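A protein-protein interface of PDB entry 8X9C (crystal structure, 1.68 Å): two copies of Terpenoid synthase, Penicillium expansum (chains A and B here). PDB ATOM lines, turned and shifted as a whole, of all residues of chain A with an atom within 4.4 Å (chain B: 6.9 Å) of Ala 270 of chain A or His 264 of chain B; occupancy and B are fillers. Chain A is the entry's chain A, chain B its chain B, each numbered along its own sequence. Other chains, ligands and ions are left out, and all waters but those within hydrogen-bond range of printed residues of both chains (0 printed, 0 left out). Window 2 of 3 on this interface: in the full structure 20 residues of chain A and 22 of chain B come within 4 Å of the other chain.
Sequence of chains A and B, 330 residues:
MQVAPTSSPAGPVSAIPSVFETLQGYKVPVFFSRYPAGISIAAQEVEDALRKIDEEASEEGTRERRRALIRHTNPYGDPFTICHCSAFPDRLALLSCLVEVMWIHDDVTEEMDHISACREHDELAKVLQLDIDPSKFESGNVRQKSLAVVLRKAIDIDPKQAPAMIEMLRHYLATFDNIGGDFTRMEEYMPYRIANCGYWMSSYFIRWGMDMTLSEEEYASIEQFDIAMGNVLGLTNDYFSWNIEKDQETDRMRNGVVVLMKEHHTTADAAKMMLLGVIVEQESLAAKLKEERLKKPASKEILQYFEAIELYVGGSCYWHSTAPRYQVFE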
ATOM      1  N   THR A 266     -18.729  -8.190  16.284  1.00  0.00           N
ATOM      2  CA  THR A 266     -18.056  -7.299  15.351  1.00  0.00           C
ATOM      3  C   THR A 266     -18.079  -7.893  13.952  1.00  0.00           C
ATOM      4  O   THR A 266     -18.463  -9.047  13.741  1.00  0.00           O
ATOM      5  CB  THR A 266     -16.597  -7.037  15.752  1.00  0.00           C
ATOM      6  OG1 THR A 266     -15.842  -8.239  15.579  1.00  0.00           O
ATOM      7  CG2 THR A 266     -16.495  -6.581  17.211  1.00  0.00           C
ATOM      8  N   THR A 267     -17.663  -7.075  12.990  1.00  0.00           N
ATOM      9  CA  THR A 267     -17.433  -7.554  11.639  1.00  0.00           C
ATOM     10  C   THR A 267     -16.255  -8.525  11.624  1.00  0.00           C
ATOM     11  O   THR A 267     -15.476  -8.610  12.578  1.00  0.00           O
ATOM     12  CB  THR A 267     -17.128  -6.395  10.697  1.00  0.00           C
ATOM     13  OG1 THR A 267     -15.917  -5.744  11.122  1.00  0.00           O
ATOM     14  CG2 THR A 267     -18.267  -5.388  10.701  1.00  0.00           C
ATOM     15  N   ALA A 268     -16.118  -9.240  10.504  1.00  0.00           N
ATOM     16  CA  ALA A 268     -14.994 -10.160  10.355  1.00  0.00           C
ATOM     17  C   ALA A 268     -13.674  -9.409  10.258  1.00  0.00           C
ATOM     18  O   ALA A 268     -12.660  -9.871  10.786  1.00  0.00           O
ATOM     19  CB  ALA A 268     -15.190 -11.060   9.137  1.00  0.00           C
ATOM     20  N   ASP A 269     -13.649  -8.256   9.583  1.00  0.00           N
ATOM     21  CA  ASP A 269     -12.395  -7.505   9.503  1.00  0.00           C
ATOM     22  C   ASP A 269     -11.948  -7.015  10.873  1.00  0.00           C
ATOM     23  O   ASP A 269     -10.749  -7.007  11.172  1.00  0.00           O
ATOM     24  CB  ASP A 269     -12.511  -6.327   8.534  1.00  0.00           C
ATOM     25  CG  ASP A 269     -12.680  -6.767   7.093  1.00  0.00           C
ATOM     26  OD1 ASP A 269     -12.428  -7.955   6.793  1.00  0.00           O
ATOM     27  OD2 ASP A 269     -13.035  -5.913   6.252  1.00  0.00           O
ATOM     28  N   ALA A 270     -12.890  -6.585  11.716  1.00  0.00           N
ATOM     29  CA  ALA A 270     -12.510  -6.147  13.055  1.00  0.00           C
ATOM     30  C   ALA A 270     -12.014  -7.319  13.888  1.00  0.00           C
ATOM     31  O   ALA A 270     -11.051  -7.188  14.650  1.00  0.00           O
ATOM     32  CB  ALA A 270     -13.687  -5.459  13.745  1.00  0.00           C
ATOM     33  N   ALA A 271     -12.672  -8.471  13.757  1.00  0.00           N
ATOM     34  CA  ALA A 271     -12.276  -9.644  14.527  1.00  0.00           C
ATOM     35  C   ALA A 271     -10.935 -10.192  14.056  1.00  0.00           C
ATOM     36  O   ALA A 271     -10.156 -10.709  14.863  1.00  0.00           O
ATOM     37  CB  ALA A 271     -13.354 -10.723  14.427  1.00  0.00           C
ATOM     38  N   LYS A 272     -10.668 -10.124  12.755  1.00  0.00           N
ATOM     39  CA  LYS A 272      -9.350 -10.578  12.244  1.00  0.00           C
ATOM     40  C   LYS A 272      -8.241  -9.685  12.807  1.00  0.00           C
ATOM     41  O   LYS A 272      -7.167 -10.192  13.123  1.00  0.00           O
ATOM     42  CB  LYS A 272      -9.295 -10.541  10.717  1.00  0.00           C
ATOM     43  CG  LYS A 272      -8.046 -11.161  10.113  1.00  0.00           C
ATOM     44  CD  LYS A 272      -8.155 -11.427   8.634  1.00  0.00           C
ATOM     45  CE  LYS A 272      -7.036 -12.301   8.115  1.00  0.00           C
ATOM     46  NZ  LYS A 272      -6.845 -12.121   6.658  1.00  0.00           N
ATOM     47  N   MET A 273      -8.523  -8.395  12.930  1.00  0.00           N
ATOM     48  CA  MET A 273      -7.525  -7.506  13.496  1.00  0.00           C
ATOM     49  C   MET A 273      -7.351  -7.813  14.978  1.00  0.00           C
ATOM     50  O   MET A 273      -6.227  -7.881  15.480  1.00  0.00           O
ATOM     51  CB  MET A 273      -7.972  -6.056  13.276  1.00  0.00           C
ATOM     52  CG  MET A 273      -7.507  -5.444  11.948  1.00  0.00           C
ATOM     53  SD  MET A 273      -5.836  -5.771  11.393  1.00  0.00           S
ATOM     54  CE  MET A 273      -6.033  -7.238  10.354  1.00  0.00           C
ATOM     55  N   MET A 274      -8.451  -8.103  15.666  1.00  0.00           N
ATOM     56  CA  MET A 274      -8.366  -8.503  17.092  1.00  0.00           C
ATOM     57  C   MET A 274      -7.566  -9.813  17.217  1.00  0.00           C
ATOM     58  O   MET A 274      -6.755  -9.907  18.130  1.00  0.00           O
ATOM     59  CB  MET A 274      -9.764  -8.702  17.686  1.00  0.00           C
ATOM     60  CG  MET A 274      -9.885  -8.341  19.139  1.00  0.00           C
ATOM     61  SD  MET A 274     -11.582  -8.643  19.673  1.00  0.00           S
ATOM     62  CE  MET A 274     -12.492  -7.815  18.373  1.00  0.00           C
ATOM     63  N   THR B 184     -15.075   8.960  15.299  1.00  0.00           N
ATOM     64  CA  THR B 184     -15.910   7.777  15.440  1.00  0.00           C
ATOM     65  C   THR B 184     -15.564   6.650  14.475  1.00  0.00           C
ATOM     66  O   THR B 184     -16.140   5.564  14.605  1.00  0.00           O
ATOM     67  CB  THR B 184     -17.398   8.136  15.264  1.00  0.00           C
ATOM     68  OG1 THR B 184     -17.643   8.537  13.905  1.00  0.00           O
ATOM     69  CG2 THR B 184     -17.788   9.264  16.197  1.00  0.00           C
ATOM     70  N   MET B 186     -11.952   4.871  12.280  1.00  0.00           N
ATOM     71  CA  MET B 186     -10.480   4.853  12.116  1.00  0.00           C
ATOM     72  C   MET B 186     -10.126   5.427  10.750  1.00  0.00           C
ATOM     73  O   MET B 186      -9.064   6.039  10.632  1.00  0.00           O
ATOM     74  CB  MET B 186      -9.971   3.416  12.216  1.00  0.00           C
ATOM     75  CG  MET B 186      -9.820   2.939  13.633  1.00  0.00           C
ATOM     76  SD  MET B 186      -8.504   3.824  14.481  1.00  0.00           S
ATOM     77  CE  MET B 186      -7.113   2.746  14.152  1.00  0.00           C
ATOM     78  N   VAL B 259     -11.282   5.346  19.620  1.00  0.00           N
ATOM     79  CA  VAL B 259     -11.947   5.336  18.323  1.00  0.00           C
ATOM     80  C   VAL B 259     -12.506   3.950  18.033  1.00  0.00           C
ATOM     81  O   VAL B 259     -13.650   3.801  17.585  1.00  0.00           O
ATOM     82  CB  VAL B 259     -10.975   5.790  17.221  1.00  0.00           C
ATOM     83  CG1 VAL B 259     -11.660   5.788  15.866  1.00  0.00           C
ATOM     84  CG2 VAL B 259     -10.405   7.174  17.541  1.00  0.00           C
ATOM     85  N   LEU B 260     -11.710   2.921  18.305  1.00  0.00           N
ATOM     86  CA  LEU B 260     -12.140   1.547  17.952  1.00  0.00           C
ATOM     87  C   LEU B 260     -13.294   1.099  18.860  1.00  0.00           C
ATOM     88  O   LEU B 260     -14.206   0.458  18.335  1.00  0.00           O
ATOM     89  CB  LEU B 260     -10.928   0.617  18.046  1.00  0.00           C
ATOM     90  CG  LEU B 260      -9.935   0.736  16.895  1.00  0.00           C
ATOM     91  CD1 LEU B 260      -8.670  -0.047  17.191  1.00  0.00           C
ATOM     92  CD2 LEU B 260     -10.562   0.264  15.597  1.00  0.00           C
ATOM     93  N   MET B 261     -13.251   1.413  20.156  1.00  0.00           N
ATOM     94  CA  MET B 261     -14.411   1.060  20.977  1.00  0.00           C
ATOM     95  C   MET B 261     -15.675   1.735  20.473  1.00  0.00           C
ATOM     96  O   MET B 261     -16.755   1.131  20.490  1.00  0.00           O
ATOM     97  CB  MET B 261     -14.231   1.380  22.470  1.00  0.00           C
ATOM     98  CG  MET B 261     -12.944   1.011  23.142  1.00  0.00           C
ATOM     99  SD  MET B 261     -12.772   1.865  24.722  1.00  0.00           S
ATOM    100  CE  MET B 261     -14.297   1.388  25.539  1.00  0.00           C
ATOM    101  N   LYS B 262     -15.572   2.985  20.022  1.00  0.00           N
ATOM    102  CA  LYS B 262     -16.772   3.677  19.565  1.00  0.00           C
ATOM    103  C   LYS B 262     -17.217   3.161  18.199  1.00  0.00           C
ATOM    104  O   LYS B 262     -18.421   3.049  17.936  1.00  0.00           O
ATOM    105  CB  LYS B 262     -16.534   5.192  19.542  1.00  0.00           C
ATOM    106  CG  LYS B 262     -16.116   5.760  20.902  1.00  0.00           C
ATOM    107  CD  LYS B 262     -16.324   7.277  21.011  1.00  0.00           C
ATOM    108  CE  LYS B 262     -15.865   8.018  19.768  1.00  0.00           C
ATOM    109  NZ  LYS B 262     -14.479   8.590  19.899  1.00  0.00           N
ATOM    110  N   GLU B 263     -16.266   2.811  17.329  1.00  0.00           N
ATOM    111  CA  GLU B 263     -16.618   2.371  15.983  1.00  0.00           C
ATOM    112  C   GLU B 263     -17.240   0.982  15.987  1.00  0.00           C
ATOM    113  O   GLU B 263     -18.189   0.719  15.241  1.00  0.00           O
ATOM    114  CB  GLU B 263     -15.394   2.384  15.073  1.00  0.00           C
ATOM    115  CG  GLU B 263     -15.747   2.066  13.633  1.00  0.00           C
ATOM    116  CD  GLU B 263     -14.584   2.176  12.675  1.00  0.00           C
ATOM    117  OE1 GLU B 263     -13.432   2.376  13.139  1.00  0.00           O
ATOM    118  OE2 GLU B 263     -14.819   2.039  11.450  1.00  0.00           O
ATOM    119  N   HIS B 264     -16.694   0.073  16.789  1.00  0.00           N
ATOM    120  CA  HIS B 264     -17.149  -1.309  16.814  1.00  0.00           C
ATOM    121  C   HIS B 264     -17.926  -1.688  18.065  1.00  0.00           C
ATOM    122  O   HIS B 264     -18.368  -2.840  18.167  1.00  0.00           O
ATOM    123  CB  HIS B 264     -15.953  -2.252  16.617  1.00  0.00           C
ATOM    124  CG  HIS B 264     -15.272  -2.067  15.303  1.00  0.00           C
ATOM    125  ND1 HIS B 264     -14.145  -1.287  15.134  1.00  0.00           N
ATOM    126  CD2 HIS B 264     -15.618  -2.495  14.067  1.00  0.00           C
ATOM    127  CE1 HIS B 264     -13.802  -1.288  13.857  1.00  0.00           C
ATOM    128  NE2 HIS B 264     -14.677  -2.017  13.190  1.00  0.00           N
ATOM    129  N   HIS B 265     -18.121  -0.758  19.003  1.00  0.00           N
ATOM    130  CA  HIS B 265     -18.928  -0.983  20.205  1.00  0.00           C
ATOM    131  C   HIS B 265     -18.406  -2.182  21.001  1.00  0.00           C
ATOM    132  O   HIS B 265     -19.125  -3.147  21.266  1.00  0.00           O
ATOM    133  CB  HIS B 265     -20.404  -1.172  19.837  1.00  0.00           C
ATOM    134  CG  HIS B 265     -20.927  -0.146  18.876  1.00  0.00           C
ATOM    135  ND1 HIS B 265     -21.089   1.181  19.213  1.00  0.00           N
ATOM    136  CD2 HIS B 265     -21.309  -0.254  17.581  1.00  0.00           C
ATOM    137  CE1 HIS B 265     -21.562   1.843  18.172  1.00  0.00           C
ATOM    138  NE2 HIS B 265     -21.704   0.996  17.168  1.00  0.00           N
ATOM    139  N   THR B 266     -17.128  -2.114  21.363  1.00  0.00           N
ATOM    140  CA  THR B 266     -16.441  -3.181  22.075  1.00  0.00           C
ATOM    141  C   THR B 266     -15.873  -2.660  23.386  1.00  0.00           C
ATOM    142  O   THR B 266     -15.886  -1.460  23.667  1.00  0.00           O
ATOM    143  CB  THR B 266     -15.308  -3.779  21.229  1.00  0.00           C
ATOM    144  OG1 THR B 266     -14.202  -2.863  21.240  1.00  0.00           O
ATOM    145  CG2 THR B 266     -15.754  -4.037  19.807  1.00  0.00           C
ATOM    146  N   THR B 267     -15.348  -3.582  24.188  1.00  0.00           N
ATOM    147  CA  THR B 267     -14.628  -3.180  25.383  1.00  0.00           C
ATOM    148  C   THR B 267     -13.281  -2.559  25.009  1.00  0.00           C
ATOM    149  O   THR B 267     -12.803  -2.671  23.874  1.00  0.00           O
ATOM    150  CB  THR B 267     -14.386  -4.368  26.300  1.00  0.00           C
ATOM    151  OG1 THR B 267     -13.628  -5.359  25.593  1.00  0.00           O
ATOM    152  CG2 THR B 267     -15.709  -4.965  26.747  1.00  0.00           C
ATOM    153  N   ALA B 270     -10.778  -5.317  24.079  1.00  0.00           N
ATOM    154  CA  ALA B 270     -10.974  -5.785  22.713  1.00  0.00           C
ATOM    155  C   ALA B 270     -10.442  -4.771  21.703  1.00  0.00           C
ATOM    156  O   ALA B 270      -9.759  -5.143  20.741  1.00  0.00           O
ATOM    157  CB  ALA B 270     -12.457  -6.074  22.469  1.00  0.00           C
ATOM    158  N   MET B 273      -6.676  -4.830  21.518  1.00  0.00           N
ATOM    159  CA  MET B 273      -6.161  -5.906  20.688  1.00  0.00           C
ATOM    160  C   MET B 273      -6.376  -5.603  19.212  1.00  0.00           C
ATOM    161  O   MET B 273      -5.505  -5.898  18.387  1.00  0.00           O
ATOM    162  CB  MET B 273      -6.804  -7.240  21.084  1.00  0.00           C
ATOM    163  CG  MET B 273      -6.279  -7.731  22.418  1.00  0.00           C
ATOM    164  SD  MET B 273      -4.547  -8.215  22.348  1.00  0.00           S
ATOM    165  CE  MET B 273      -3.764  -6.771  23.088  1.00  0.00           C
ATOM    166  N   MET B 274      -7.504  -4.990  18.877  1.00  0.00           N
ATOM    167  CA  MET B 274      -7.755  -4.593  17.468  1.00  0.00           C
ATOM    168  C   MET B 274      -6.703  -3.570  17.011  1.00  0.00           C
ATOM    169  O   MET B 274      -6.225  -3.687  15.882  1.00  0.00           O
ATOM    170  CB  MET B 274      -9.154  -3.991  17.330  1.00  0.00           C
ATOM    171  CG  MET B 274      -9.868  -4.343  16.054  1.00  0.00           C
ATOM    172  SD  MET B 274     -11.505  -3.572  16.036  1.00  0.00           S
ATOM    173  CE  MET B 274     -12.171  -4.186  17.580  1.00  0.00           C
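Hydrophobic or aromatic side chains of chain A within 4 Å of the printed part of chain B: Ala 270, Met 273 and Met 274. Among the printed residues, no Asp or Glu carboxylate lies within 4 Å of a Lys or Arg side-chain nitrogen of the other chain.
Thr 266 of chain B touches its own counterpart, Thr 266 of chain A. Ala 270 of chain A touches Met 274 of chain B, and with the chains exchanged Met 274 of chain A touches Ala 270 of chain B. Met 273 of chain A touches its own counterpart, Met 273 of chain B. Met 274 of chain A touches its own counterpart, Met 274 of chain B. Of the 8 pairs that touch across the chains among the printed residues, 7 have their exchanged pair printed and touching as well.
Among the printed residues, pairs that only touch across the chains: Ala 270 of chain A with Met 274 of chain B (3.4 Å), Ala 270 of chain A with His 264 of chain B (3.6 Å), Met 274 of chain A with Ala 270 of chain B (3.6 Å), Met 273 of chain A with Met 273 of chain B (3.6 Å), Thr 266 of chain A with Thr 266 of chain B (3.7 Å), Met 274 of chain A with Met 274 of chain B (3.7 Å), Met 273 of chain A with Met 274 of chain B (3.8 Å) and Met 274 of chain A with Met 273 of chain B (3.8 Å).
The side-chain hydroxyl of Thr 267 of chain A lies within hydrogen-bond range of the backbone NH of Ala 270 of chain A (3.2 Å). A ring nitrogen (ND1) of His 264 of chain B lies within hydrogen-bond range of the side-chain sulfur (SD) of Met 274 of chain B, 3.6 Å away. OG1 of Thr 267 of chain B lies within hydrogen-bond range of N of Ala 270 of chain B, 3.2 Å away. N of Thr 266 of chain B is in hydrogen-bond range of O of Met 261 of chain B (3.4 Å).
Ala 270 of chain A touches two residues of chain B. Printed residues of chain B within 4 Å of Met 274 of chain A: Ala 270, Met 273 and Met 274. Of the printed residues of chain A, Thr 266 of chain B touches Thr 266. Of the printed residues of chain A, Ala 270 of chain B touches Met 274. Of the printed residues of chain A, Met 273 of chain B touches Met 273 (3.6 Å) and Met 274 (3.8 Å). Printed residues of chain A within 4 Å of Met 274 of chain B: Ala 270, Met 273 and Met 274. The nearest printed residue of chain B that does not touch Ala 270 of chain A is Ala 270 of chain B (6.6 Å).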
